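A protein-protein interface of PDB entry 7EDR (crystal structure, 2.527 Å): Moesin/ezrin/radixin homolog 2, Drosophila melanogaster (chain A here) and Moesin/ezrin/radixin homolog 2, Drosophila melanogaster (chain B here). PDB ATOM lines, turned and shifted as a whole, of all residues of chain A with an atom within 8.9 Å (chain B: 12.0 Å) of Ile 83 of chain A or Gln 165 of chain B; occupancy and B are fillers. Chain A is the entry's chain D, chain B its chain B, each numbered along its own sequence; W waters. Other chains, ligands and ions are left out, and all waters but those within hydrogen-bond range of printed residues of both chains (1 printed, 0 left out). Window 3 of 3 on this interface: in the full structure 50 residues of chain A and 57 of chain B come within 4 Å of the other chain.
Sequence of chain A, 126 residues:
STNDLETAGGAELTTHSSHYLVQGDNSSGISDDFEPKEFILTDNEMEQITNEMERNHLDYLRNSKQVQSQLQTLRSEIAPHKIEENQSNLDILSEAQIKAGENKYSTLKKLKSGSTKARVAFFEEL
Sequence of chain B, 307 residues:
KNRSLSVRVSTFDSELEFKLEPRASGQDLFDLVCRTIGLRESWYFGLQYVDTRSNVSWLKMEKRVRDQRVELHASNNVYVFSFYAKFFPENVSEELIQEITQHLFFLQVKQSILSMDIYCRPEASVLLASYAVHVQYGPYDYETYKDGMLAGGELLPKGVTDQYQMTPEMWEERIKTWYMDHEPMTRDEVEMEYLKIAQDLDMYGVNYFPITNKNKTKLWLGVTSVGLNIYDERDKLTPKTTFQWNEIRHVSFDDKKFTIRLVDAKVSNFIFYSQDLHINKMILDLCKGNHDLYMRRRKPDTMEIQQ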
ATOM      1  N   ILE A  78      27.100  12.990 -21.721  1.00  0.00           N
ATOM      2  CA  ILE A  78      27.161  11.591 -22.142  1.00  0.00           C
ATOM      3  C   ILE A  78      28.141  11.375 -23.289  1.00  0.00           C
ATOM      4  O   ILE A  78      28.498  10.217 -23.574  1.00  0.00           O
ATOM      5  CB  ILE A  78      25.776  11.026 -22.539  1.00  0.00           C
ATOM      6  CG1 ILE A  78      25.192  11.793 -23.725  1.00  0.00           C
ATOM      7  CG2 ILE A  78      24.804  11.058 -21.356  1.00  0.00           C
ATOM      8  CD1 ILE A  78      23.967  11.161 -24.280  1.00  0.00           C
ATOM      9  N   ALA A  79      28.604  12.446 -23.939  1.00  0.00           N
ATOM     10  CA  ALA A  79      29.505  12.316 -25.089  1.00  0.00           C
ATOM     11  C   ALA A  79      30.724  11.410 -24.861  1.00  0.00           C
ATOM     12  O   ALA A  79      31.062  10.640 -25.779  1.00  0.00           O
ATOM     13  CB  ALA A  79      29.958  13.715 -25.540  1.00  0.00           C
ATOM     14  N   PRO A  80      31.418  11.440 -23.714  1.00  0.00           N
ATOM     15  CA  PRO A  80      32.549  10.506 -23.528  1.00  0.00           C
ATOM     16  C   PRO A  80      32.183   9.037 -23.692  1.00  0.00           C
ATOM     17  O   PRO A  80      33.069   8.223 -23.977  1.00  0.00           O
ATOM     18  CB  PRO A  80      33.020  10.795 -22.094  1.00  0.00           C
ATOM     19  CG  PRO A  80      32.525  12.174 -21.785  1.00  0.00           C
ATOM     20  CD  PRO A  80      31.241  12.335 -22.549  1.00  0.00           C
ATOM     21  N   HIS A  81      30.920   8.659 -23.517  1.00  0.00           N
ATOM     22  CA  HIS A  81      30.524   7.261 -23.635  1.00  0.00           C
ATOM     23  C   HIS A  81      30.101   6.869 -25.041  1.00  0.00           C
ATOM     24  O   HIS A  81      29.601   5.754 -25.223  1.00  0.00           O
ATOM     25  CB  HIS A  81      29.392   6.959 -22.664  1.00  0.00           C
ATOM     26  CG  HIS A  81      29.719   7.326 -21.256  1.00  0.00           C
ATOM     27  ND1 HIS A  81      30.711   6.690 -20.540  1.00  0.00           N
ATOM     28  CD2 HIS A  81      29.216   8.282 -20.441  1.00  0.00           C
ATOM     29  CE1 HIS A  81      30.790   7.227 -19.337  1.00  0.00           C
ATOM     30  NE2 HIS A  81      29.892   8.192 -19.252  1.00  0.00           N
ATOM     31  N   LYS A  82      30.299   7.747 -26.024  1.00  0.00           N
ATOM     32  CA  LYS A  82      29.849   7.507 -27.388  1.00  0.00           C
ATOM     33  C   LYS A  82      30.596   6.342 -28.024  1.00  0.00           C
ATOM     34  O   LYS A  82      31.816   6.214 -27.897  1.00  0.00           O
ATOM     35  CB  LYS A  82      30.042   8.768 -28.230  1.00  0.00           C
ATOM     36  CG  LYS A  82      29.579   8.635 -29.669  1.00  0.00           C
ATOM     37  CD  LYS A  82      28.479   9.637 -29.963  1.00  0.00           C
ATOM     38  CE  LYS A  82      28.981  11.059 -29.772  1.00  0.00           C
ATOM     39  NZ  LYS A  82      29.920  11.436 -30.865  1.00  0.00           N
ATOM     40  N   ILE A  83      29.861   5.490 -28.717  1.00  0.00           N
ATOM     41  CA  ILE A  83      30.455   4.416 -29.501  1.00  0.00           C
ATOM     42  C   ILE A  83      30.312   4.830 -30.959  1.00  0.00           C
ATOM     43  O   ILE A  83      29.264   4.604 -31.575  1.00  0.00           O
ATOM     44  CB  ILE A  83      29.786   3.069 -29.225  1.00  0.00           C
ATOM     45  CG1 ILE A  83      29.747   2.784 -27.718  1.00  0.00           C
ATOM     46  CG2 ILE A  83      30.497   1.975 -29.967  1.00  0.00           C
ATOM     47  CD1 ILE A  83      28.918   1.557 -27.342  1.00  0.00           C
ATOM     48  N   GLU A  84      31.366   5.437 -31.520  1.00  0.00           N
ATOM     49  CA  GLU A  84      31.257   6.055 -32.842  1.00  0.00           C
ATOM     50  C   GLU A  84      30.966   5.033 -33.936  1.00  0.00           C
ATOM     51  O   GLU A  84      30.151   5.286 -34.826  1.00  0.00           O
ATOM     52  CB  GLU A  84      32.526   6.830 -33.158  1.00  0.00           C
ATOM     53  CG  GLU A  84      32.735   8.000 -32.238  1.00  0.00           C
ATOM     54  CD  GLU A  84      33.728   8.994 -32.794  1.00  0.00           C
ATOM     55  OE1 GLU A  84      34.071   8.863 -33.992  1.00  0.00           O
ATOM     56  OE2 GLU A  84      34.162   9.898 -32.037  1.00  0.00           O
ATOM     57  N   GLU A  85      31.606   3.872 -33.883  1.00  0.00           N
ATOM     58  CA  GLU A  85      31.344   2.801 -34.841  1.00  0.00           C
ATOM     59  C   GLU A  85      29.910   2.281 -34.747  1.00  0.00           C
ATOM     60  O   GLU A  85      29.511   1.389 -35.503  1.00  0.00           O
ATOM     61  CB  GLU A  85      32.337   1.650 -34.632  1.00  0.00           C
ATOM     62  CG  GLU A  85      32.597   1.292 -33.163  1.00  0.00           C
ATOM     63  CD  GLU A  85      33.590   2.250 -32.485  1.00  0.00           C
ATOM     64  OE1 GLU A  85      34.240   3.053 -33.205  1.00  0.00           O
ATOM     65  OE2 GLU A  85      33.710   2.223 -31.235  1.00  0.00           O
ATOM     66  N   ASN A  86      29.122   2.825 -33.821  1.00  0.00           N
ATOM     67  CA  ASN A  86      27.729   2.436 -33.672  1.00  0.00           C
ATOM     68  C   ASN A  86      26.757   3.528 -34.098  1.00  0.00           C
ATOM     69  O   ASN A  86      25.540   3.313 -34.033  1.00  0.00           O
ATOM     70  CB  ASN A  86      27.450   2.015 -32.226  1.00  0.00           C
ATOM     71  CG  ASN A  86      27.892   0.594 -31.941  1.00  0.00           C
ATOM     72  OD1 ASN A  86      28.659   0.007 -32.704  1.00  0.00           O
ATOM     73  ND2 ASN A  86      27.397   0.026 -30.844  1.00  0.00           N
ATOM     74  N   GLN A  87      27.261   4.680 -34.544  1.00  0.00           N
ATOM     75  CA  GLN A  87      26.420   5.769 -35.010  1.00  0.00           C
ATOM     76  C   GLN A  87      25.866   5.475 -36.396  1.00  0.00           C
ATOM     77  O   GLN A  87      26.577   4.954 -37.266  1.00  0.00           O
ATOM     78  CB  GLN A  87      27.220   7.064 -35.052  1.00  0.00           C
ATOM     79  CG  GLN A  87      27.853   7.424 -33.745  1.00  0.00           C
ATOM     80  CD  GLN A  87      28.075   8.908 -33.640  1.00  0.00           C
ATOM     81  OE1 GLN A  87      27.275   9.620 -33.025  1.00  0.00           O
ATOM     82  NE2 GLN A  87      29.147   9.396 -34.261  1.00  0.00           N
ATOM     83  N   SER A  88      24.596   5.831 -36.607  1.00  0.00           N
ATOM     84  CA  SER A  88      23.975   5.693 -37.918  1.00  0.00           C
ATOM     85  C   SER A  88      24.295   6.905 -38.793  1.00  0.00           C
ATOM     86  O   SER A  88      24.714   7.964 -38.312  1.00  0.00           O
ATOM     87  CB  SER A  88      22.461   5.546 -37.793  1.00  0.00           C
ATOM     88  OG  SER A  88      21.850   6.824 -37.630  1.00  0.00           O
ATOM     89  N   ASP A  91      22.772   9.957 -37.573  1.00  0.00           N
ATOM     90  CA  ASP A  91      23.503  10.556 -36.452  1.00  0.00           C
ATOM     91  C   ASP A  91      24.630  11.442 -36.947  1.00  0.00           C
ATOM     92  O   ASP A  91      24.855  12.538 -36.417  1.00  0.00           O
ATOM     93  CB  ASP A  91      24.077   9.464 -35.544  1.00  0.00           C
ATOM     94  CG  ASP A  91      23.006   8.737 -34.747  1.00  0.00           C
ATOM     95  OD1 ASP A  91      22.219   9.433 -34.066  1.00  0.00           O
ATOM     96  OD2 ASP A  91      22.949   7.479 -34.809  1.00  0.00           O
ATOM     97  N   GLU A  95      24.734  15.421 -36.348  1.00  0.00           N
ATOM     98  CA  GLU A  95      25.813  16.134 -35.667  1.00  0.00           C
ATOM     99  C   GLU A  95      26.385  17.237 -36.546  1.00  0.00           C
ATOM    100  O   GLU A  95      26.640  18.352 -36.069  1.00  0.00           O
ATOM    101  CB  GLU A  95      26.910  15.154 -35.223  1.00  0.00           C
ATOM    102  CG  GLU A  95      26.616  14.455 -33.890  1.00  0.00           C
ATOM    103  CD  GLU A  95      27.460  13.194 -33.652  1.00  0.00           C
ATOM    104  OE1 GLU A  95      28.424  12.954 -34.416  1.00  0.00           O
ATOM    105  OE2 GLU A  95      27.148  12.422 -32.703  1.00  0.00           O
ATOM    106  N   TYR B 119      13.783   9.968 -37.016  1.00  0.00           N
ATOM    107  CA  TYR B 119      15.012  10.069 -36.253  1.00  0.00           C
ATOM    108  C   TYR B 119      14.855  11.068 -35.117  1.00  0.00           C
ATOM    109  O   TYR B 119      14.114  12.050 -35.214  1.00  0.00           O
ATOM    110  CB  TYR B 119      16.163  10.486 -37.162  1.00  0.00           C
ATOM    111  CG  TYR B 119      17.427  10.853 -36.429  1.00  0.00           C
ATOM    112  CD1 TYR B 119      18.343   9.866 -36.041  1.00  0.00           C
ATOM    113  CD2 TYR B 119      17.720  12.185 -36.126  1.00  0.00           C
ATOM    114  CE1 TYR B 119      19.509  10.190 -35.380  1.00  0.00           C
ATOM    115  CE2 TYR B 119      18.883  12.517 -35.460  1.00  0.00           C
ATOM    116  CZ  TYR B 119      19.778  11.509 -35.090  1.00  0.00           C
ATOM    117  OH  TYR B 119      20.941  11.823 -34.415  1.00  0.00           O
ATOM    118  N   ARG B 121      17.474  12.819 -31.802  1.00  0.00           N
ATOM    119  CA  ARG B 121      18.801  12.888 -31.209  1.00  0.00           C
ATOM    120  C   ARG B 121      18.803  12.267 -29.813  1.00  0.00           C
ATOM    121  O   ARG B 121      17.778  12.276 -29.123  1.00  0.00           O
ATOM    122  CB  ARG B 121      19.288  14.334 -31.127  1.00  0.00           C
ATOM    123  CG  ARG B 121      19.808  14.893 -32.459  1.00  0.00           C
ATOM    124  CD  ARG B 121      20.791  16.051 -32.267  1.00  0.00           C
ATOM    125  NE  ARG B 121      21.846  15.737 -31.297  1.00  0.00           N
ATOM    126  CZ  ARG B 121      22.922  14.980 -31.539  1.00  0.00           C
ATOM    127  NH1 ARG B 121      23.120  14.435 -32.736  1.00  0.00           N
ATOM    128  NH2 ARG B 121      23.800  14.758 -30.565  1.00  0.00           N
ATOM    129  N   PRO B 122      19.943  11.708 -29.387  1.00  0.00           N
ATOM    130  CA  PRO B 122      19.986  11.057 -28.062  1.00  0.00           C
ATOM    131  C   PRO B 122      19.504  11.948 -26.927  1.00  0.00           C
ATOM    132  O   PRO B 122      18.637  11.534 -26.150  1.00  0.00           O
ATOM    133  CB  PRO B 122      21.473  10.674 -27.912  1.00  0.00           C
ATOM    134  CG  PRO B 122      21.976  10.532 -29.321  1.00  0.00           C
ATOM    135  CD  PRO B 122      21.195  11.517 -30.149  1.00  0.00           C
ATOM    136  N   LEU B 156      13.636   4.671 -24.535  1.00  0.00           N
ATOM    137  CA  LEU B 156      14.565   5.259 -25.455  1.00  0.00           C
ATOM    138  C   LEU B 156      14.605   4.464 -26.746  1.00  0.00           C
ATOM    139  O   LEU B 156      14.507   3.230 -26.721  1.00  0.00           O
ATOM    140  CB  LEU B 156      15.970   5.324 -24.838  1.00  0.00           C
ATOM    141  CG  LEU B 156      16.040   6.256 -23.627  1.00  0.00           C
ATOM    142  CD1 LEU B 156      17.448   6.285 -23.015  1.00  0.00           C
ATOM    143  CD2 LEU B 156      15.559   7.672 -24.005  1.00  0.00           C
ATOM    144  N   PRO B 157      14.713   5.139 -27.889  1.00  0.00           N
ATOM    145  CA  PRO B 157      14.981   4.426 -29.143  1.00  0.00           C
ATOM    146  C   PRO B 157      16.225   3.549 -29.012  1.00  0.00           C
ATOM    147  O   PRO B 157      17.249   3.959 -28.451  1.00  0.00           O
ATOM    148  CB  PRO B 157      15.200   5.558 -30.156  1.00  0.00           C
ATOM    149  CG  PRO B 157      14.616   6.770 -29.541  1.00  0.00           C
ATOM    150  CD  PRO B 157      14.680   6.599 -28.059  1.00  0.00           C
ATOM    151  N   LYS B 158      16.144   2.332 -29.547  1.00  0.00           N
ATOM    152  CA  LYS B 158      17.303   1.443 -29.482  1.00  0.00           C
ATOM    153  C   LYS B 158      18.525   2.052 -30.162  1.00  0.00           C
ATOM    154  O   LYS B 158      19.655   1.817 -29.721  1.00  0.00           O
ATOM    155  CB  LYS B 158      16.973   0.085 -30.095  1.00  0.00           C
ATOM    156  CG  LYS B 158      18.137  -0.881 -30.037  1.00  0.00           C
ATOM    157  CD  LYS B 158      17.707  -2.335 -30.159  1.00  0.00           C
ATOM    158  CE  LYS B 158      18.856  -3.260 -29.776  1.00  0.00           C
ATOM    159  NZ  LYS B 158      20.012  -3.110 -30.715  1.00  0.00           N
ATOM    160  N   GLY B 159      18.328   2.848 -31.216  1.00  0.00           N
ATOM    161  CA  GLY B 159      19.450   3.532 -31.833  1.00  0.00           C
ATOM    162  C   GLY B 159      20.142   4.516 -30.914  1.00  0.00           C
ATOM    163  O   GLY B 159      21.307   4.871 -31.149  1.00  0.00           O
ATOM    164  N   VAL B 160      19.448   4.993 -29.884  1.00  0.00           N
ATOM    165  CA  VAL B 160      20.099   5.842 -28.896  1.00  0.00           C
ATOM    166  C   VAL B 160      20.975   5.007 -27.976  1.00  0.00           C
ATOM    167  O   VAL B 160      22.176   5.256 -27.837  1.00  0.00           O
ATOM    168  CB  VAL B 160      19.055   6.650 -28.109  1.00  0.00           C
ATOM    169  CG1 VAL B 160      19.717   7.378 -26.925  1.00  0.00           C
ATOM    170  CG2 VAL B 160      18.425   7.637 -29.021  1.00  0.00           C
ATOM    171  N   THR B 161      20.390   3.987 -27.355  1.00  0.00           N
ATOM    172  CA  THR B 161      21.118   3.230 -26.346  1.00  0.00           C
ATOM    173  C   THR B 161      22.257   2.404 -26.949  1.00  0.00           C
ATOM    174  O   THR B 161      23.271   2.193 -26.276  1.00  0.00           O
ATOM    175  CB  THR B 161      20.142   2.354 -25.555  1.00  0.00           C
ATOM    176  OG1 THR B 161      19.377   1.542 -26.454  1.00  0.00           O
ATOM    177  CG2 THR B 161      19.194   3.233 -24.744  1.00  0.00           C
ATOM    178  N   ASP B 162      22.127   1.947 -28.204  1.00  0.00           N
ATOM    179  CA  ASP B 162      23.234   1.275 -28.890  1.00  0.00           C
ATOM    180  C   ASP B 162      24.423   2.190 -29.121  1.00  0.00           C
ATOM    181  O   ASP B 162      25.542   1.704 -29.303  1.00  0.00           O
ATOM    182  CB  ASP B 162      22.809   0.747 -30.266  1.00  0.00           C
ATOM    183  CG  ASP B 162      21.783  -0.366 -30.192  1.00  0.00           C
ATOM    184  OD1 ASP B 162      21.145  -0.619 -31.228  1.00  0.00           O
ATOM    185  OD2 ASP B 162      21.600  -0.977 -29.120  1.00  0.00           O
ATOM    186  N   GLN B 163      24.199   3.490 -29.150  1.00  0.00           N
ATOM    187  CA  GLN B 163      25.202   4.478 -29.512  1.00  0.00           C
ATOM    188  C   GLN B 163      26.152   4.812 -28.365  1.00  0.00           C
ATOM    189  O   GLN B 163      27.174   5.474 -28.589  1.00  0.00           O
ATOM    190  CB  GLN B 163      24.462   5.733 -29.984  1.00  0.00           C
ATOM    191  CG  GLN B 163      25.215   6.696 -30.838  1.00  0.00           C
ATOM    192  CD  GLN B 163      24.275   7.733 -31.405  1.00  0.00           C
ATOM    193  OE1 GLN B 163      23.103   7.432 -31.669  1.00  0.00           O
ATOM    194  NE2 GLN B 163      24.766   8.957 -31.580  1.00  0.00           N
ATOM    195  N   TYR B 164      25.846   4.382 -27.146  1.00  0.00           N
ATOM    196  CA  TYR B 164      26.607   4.810 -25.983  1.00  0.00           C
ATOM    197  C   TYR B 164      26.976   3.623 -25.109  1.00  0.00           C
ATOM    198  O   TYR B 164      26.221   2.651 -24.998  1.00  0.00           O
ATOM    199  CB  TYR B 164      25.833   5.828 -25.145  1.00  0.00           C
ATOM    200  CG  TYR B 164      25.665   7.149 -25.837  1.00  0.00           C
ATOM    201  CD1 TYR B 164      24.631   7.354 -26.760  1.00  0.00           C
ATOM    202  CD2 TYR B 164      26.542   8.201 -25.580  1.00  0.00           C
ATOM    203  CE1 TYR B 164      24.479   8.573 -27.405  1.00  0.00           C
ATOM    204  CE2 TYR B 164      26.392   9.430 -26.216  1.00  0.00           C
ATOM    205  CZ  TYR B 164      25.359   9.607 -27.124  1.00  0.00           C
ATOM    206  OH  TYR B 164      25.228  10.816 -27.749  1.00  0.00           O
ATOM    207  N   GLN B 165      28.156   3.732 -24.488  1.00  0.00           N
ATOM    208  CA  GLN B 165      28.640   2.782 -23.487  1.00  0.00           C
ATOM    209  C   GLN B 165      28.047   3.163 -22.140  1.00  0.00           C
ATOM    210  O   GLN B 165      28.687   3.794 -21.295  1.00  0.00           O
ATOM    211  CB  GLN B 165      30.160   2.794 -23.427  1.00  0.00           C
ATOM    212  CG  GLN B 165      30.803   1.711 -24.229  1.00  0.00           C
ATOM    213  CD  GLN B 165      30.941   0.451 -23.434  1.00  0.00           C
ATOM    214  OE1 GLN B 165      30.180  -0.504 -23.626  1.00  0.00           O
ATOM    215  NE2 GLN B 165      31.925   0.429 -22.530  1.00  0.00           N
ATOM    216  N   MET B 166      26.791   2.776 -21.944  1.00  0.00           N
ATOM    217  CA  MET B 166      26.067   3.114 -20.728  1.00  0.00           C
ATOM    218  C   MET B 166      25.105   1.978 -20.428  1.00  0.00           C
ATOM    219  O   MET B 166      24.655   1.277 -21.336  1.00  0.00           O
ATOM    220  CB  MET B 166      25.308   4.437 -20.863  1.00  0.00           C
ATOM    221  CG  MET B 166      26.183   5.671 -20.951  1.00  0.00           C
ATOM    222  SD  MET B 166      25.258   7.129 -21.528  1.00  0.00           S
ATOM    223  CE  MET B 166      23.824   7.009 -20.455  1.00  0.00           C
ATOM    224  N   THR B 167      24.833   1.771 -19.154  1.00  0.00           N
ATOM    225  CA  THR B 167      23.888   0.739 -18.776  1.00  0.00           C
ATOM    226  C   THR B 167      22.488   1.320 -18.786  1.00  0.00           C
ATOM    227  O   THR B 167      22.317   2.541 -18.709  1.00  0.00           O
ATOM    228  CB  THR B 167      24.207   0.197 -17.376  1.00  0.00           C
ATOM    229  OG1 THR B 167      23.898   1.197 -16.392  1.00  0.00           O
ATOM    230  CG2 THR B 167      25.673  -0.195 -17.264  1.00  0.00           C
ATOM    231  N   PRO B 168      21.465   0.472 -18.884  1.00  0.00           N
ATOM    232  CA  PRO B 168      20.089   0.965 -18.727  1.00  0.00           C
ATOM    233  C   PRO B 168      19.876   1.793 -17.469  1.00  0.00           C
ATOM    234  O   PRO B 168      19.118   2.774 -17.508  1.00  0.00           O
ATOM    235  CB  PRO B 168      19.267  -0.329 -18.700  1.00  0.00           C
ATOM    236  CG  PRO B 168      20.063  -1.272 -19.542  1.00  0.00           C
ATOM    237  CD  PRO B 168      21.506  -0.957 -19.253  1.00  0.00           C
ATOM    238  N   GLU B 169      20.540   1.453 -16.360  1.00  0.00           N
ATOM    239  CA  GLU B 169      20.310   2.188 -15.119  1.00  0.00           C
ATOM    240  C   GLU B 169      20.901   3.582 -15.187  1.00  0.00           C
ATOM    241  O   GLU B 169      20.393   4.507 -14.536  1.00  0.00           O
ATOM    242  CB  GLU B 169      20.904   1.432 -13.931  1.00  0.00           C
ATOM    243  CG  GLU B 169      20.211   0.102 -13.635  1.00  0.00           C
ATOM    244  CD  GLU B 169      20.566  -1.042 -14.622  1.00  0.00           C
ATOM    245  OE1 GLU B 169      21.501  -0.922 -15.464  1.00  0.00           O
ATOM    246  OE2 GLU B 169      19.886  -2.086 -14.537  1.00  0.00           O
ATOM    247  N   MET B 170      21.985   3.743 -15.953  1.00  0.00           N
ATOM    248  CA  MET B 170      22.578   5.061 -16.118  1.00  0.00           C
ATOM    249  C   MET B 170      21.668   5.958 -16.942  1.00  0.00           C
ATOM    250  O   MET B 170      21.520   7.151 -16.639  1.00  0.00           O
ATOM    251  CB  MET B 170      23.956   4.939 -16.775  1.00  0.00           C
ATOM    252  CG  MET B 170      25.058   4.512 -15.831  1.00  0.00           C
ATOM    253  SD  MET B 170      26.502   3.805 -16.662  1.00  0.00           S
ATOM    254  CE  MET B 170      27.331   5.281 -17.289  1.00  0.00           C
ATOM    255  N   TRP B 171      21.051   5.399 -17.990  1.00  0.00           N
ATOM    256  CA  TRP B 171      20.037   6.148 -18.731  1.00  0.00           C
ATOM    257  C   TRP B 171      18.845   6.493 -17.838  1.00  0.00           C
ATOM    258  O   TRP B 171      18.408   7.650 -17.775  1.00  0.00           O
ATOM    259  CB  TRP B 171      19.571   5.349 -19.946  1.00  0.00           C
ATOM    260  CG  TRP B 171      20.519   5.277 -21.114  1.00  0.00           C
ATOM    261  CD1 TRP B 171      21.149   4.166 -21.581  1.00  0.00           C
ATOM    262  CD2 TRP B 171      20.902   6.354 -21.991  1.00  0.00           C
ATOM    263  NE1 TRP B 171      21.916   4.479 -22.682  1.00  0.00           N
ATOM    264  CE2 TRP B 171      21.781   5.815 -22.956  1.00  0.00           C
ATOM    265  CE3 TRP B 171      20.595   7.717 -22.048  1.00  0.00           C
ATOM    266  CZ2 TRP B 171      22.355   6.589 -23.972  1.00  0.00           C
ATOM    267  CZ3 TRP B 171      21.178   8.497 -23.067  1.00  0.00           C
ATOM    268  CH2 TRP B 171      22.048   7.926 -24.005  1.00  0.00           C
ATOM    269  N   GLU B 172      18.315   5.495 -17.122  1.00  0.00           N
ATOM    270  CA  GLU B 172      17.157   5.722 -16.262  1.00  0.00           C
ATOM    271  C   GLU B 172      17.411   6.839 -15.255  1.00  0.00           C
ATOM    272  O   GLU B 172      16.523   7.659 -14.995  1.00  0.00           O
ATOM    273  CB  GLU B 172      16.771   4.419 -15.557  1.00  0.00           C
ATOM    274  CG  GLU B 172      16.242   3.349 -16.519  1.00  0.00           C
ATOM    275  CD  GLU B 172      16.430   1.914 -16.026  1.00  0.00           C
ATOM    276  OE1 GLU B 172      16.402   0.997 -16.883  1.00  0.00           O
ATOM    277  OE2 GLU B 172      16.590   1.699 -14.795  1.00  0.00           O
ATOM    278  N   ARG B 174      19.290   9.488 -15.542  1.00  0.00           N
ATOM    279  CA  ARG B 174      19.207  10.776 -16.218  1.00  0.00           C
ATOM    280  C   ARG B 174      17.771  11.132 -16.606  1.00  0.00           C
ATOM    281  O   ARG B 174      17.387  12.303 -16.521  1.00  0.00           O
ATOM    282  CB  ARG B 174      20.130  10.770 -17.426  1.00  0.00           C
ATOM    283  CG  ARG B 174      21.549  10.585 -16.990  1.00  0.00           C
ATOM    284  CD  ARG B 174      22.463  10.663 -18.149  1.00  0.00           C
ATOM    285  NE  ARG B 174      23.422  11.735 -17.940  1.00  0.00           N
ATOM    286  CZ  ARG B 174      24.668  11.527 -17.563  1.00  0.00           C
ATOM    287  NH1 ARG B 174      25.085  10.278 -17.361  1.00  0.00           N
ATOM    288  NH2 ARG B 174      25.484  12.554 -17.407  1.00  0.00           N
HETATM  289  O   HOH W   1      24.152  11.596 -32.554  1.00  0.00           O
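OH of Tyr 119 of chain B sits at hydrogen-bond distance from OD1 of Asp 91 of chain A, 2.7 Å away. O of Asp 162 of chain B sits at hydrogen-bond distance from ND2 of Asn 86 of chain A (2.9 Å). The backbone carbonyl oxygen (O) of Gln 163 of chain B lies within hydrogen-bond range of the backbone NH (N) of Ile 83 of chain A, 2.7 Å away. The side-chain amide nitrogen (NE2) of Gln 163 of chain B sits at hydrogen-bond distance from the side-chain amide oxygen (OE1) of Gln 87 of chain A, 3.0 Å away. OE1 of Gln 163 of chain B lies close to OD2 of Asp 91 of chain A, at 3.1 Å. The backbone carbonyl oxygen (O) of His 81 of chain A sits at hydrogen-bond distance from the backbone NH (N) of Gln 165 of chain B, 2.6 Å away.
The side-chain amino group (NZ) of Lys 158 of chain B lies within salt-bridge range of the side-chain carboxylate (OD1) of Asp 162 of chain B (2.8 Å). O of Gly 159 of chain B sits close to OE1 of Gln 163 of chain B (3.2 Å). The side-chain amino group of Lys 82 of chain A is in salt-bridge range of the side-chain carboxylate of Glu 95 of chain A. The side-chain amide oxygen of Gln 87 of chain A sits close to the side-chain carboxylate of Glu 95 of chain A (2.8 Å). The side-chain carboxylate (OD2) of Asp 91 of chain A sits at hydrogen-bond distance from the backbone NH (N) of Ser 88 of chain A.
Among the printed residues, pairs that only touch across the chains: His 81 of chain A with Tyr 164 of chain B (3.2 Å), Ile 78 of chain A with Tyr 164 of chain B (3.5 Å), Lys 82 of chain A with Gln 163 of chain B (3.6 Å), Ile 83 of chain A with Tyr 164 of chain B (3.6 Å), Ile 83 of chain A with Gln 165 of chain B (3.6 Å), Glu 95 of chain A with Arg 121 of chain B (3.7 Å), Ile 78 of chain A with Arg 174 of chain B (3.7 Å), Ile 78 of chain A with Trp 171 of chain B (3.8 Å), Lys 82 of chain A with Tyr 164 of chain B (3.8 Å), His 81 of chain A with Met 166 of chain B (3.9 Å), Ile 83 of chain A with Asp 162 of chain B (3.9 Å) and Ile 78 of chain A with Met 166 of chain B (3.96 Å).
His 81 of chain A touches just these residues of chain B: Tyr 164 (3.2 Å), Gln 165 (2.6 Å) and Met 166 (3.9 Å). Ile 83 of chain A touches just these residues of chain B: Asp 162 (3.9 Å), Gln 163 (2.7 Å), Tyr 164 (3.6 Å) and Gln 165 (3.6 Å). Of chain B, only Asp 162 comes within 4 Å of Asn 86 of chain A. Of chain B, only Gln 163 comes within 4 Å of Gln 87 of chain A. Of the printed residues of chain B, Asp 91 of chain A touches Tyr 119 and Gln 163. Thr 161 of chain B touches none of the printed residues of chain A. Gln 165 of chain B touches just these residues of chain A: His 81 and Ile 83. Met 170 of chain B touches none of the printed residues of chain A. Of the printed residues of chain A, Arg 174 of chain B touches Ile 78 (3.7 Å). The nearest residue of chain A that does not touch Gln 165 of chain B is Lys 82 of chain A (4.8 Å).
Of the 13 printed residues of chain A, 8 touch a printed residue of chain B. Of the 21 printed residues of chain B, 9 touch a printed residue of chain A. Printed residues of chain B that touch a printed residue of chain A: Tyr 119, Arg 121, Asp 162, Gln 163, Tyr 164, Gln 165, Met 166, Trp 171 and Arg 174. Hydrophobic or aromatic side chains of chain B that line the printed part of chain A: Tyr 119, Tyr 164, Met 166 and Trp 171.
Water W1 lies within hydrogen-bond range of NE2 of Gln 163 of chain B (2.9 Å), NH1 of Arg 121 of chain B (3.0 Å), OE2 of Glu 95 of chain A (3.1 Å) and OD1 of Asp 91 of chain A (3.3 Å).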
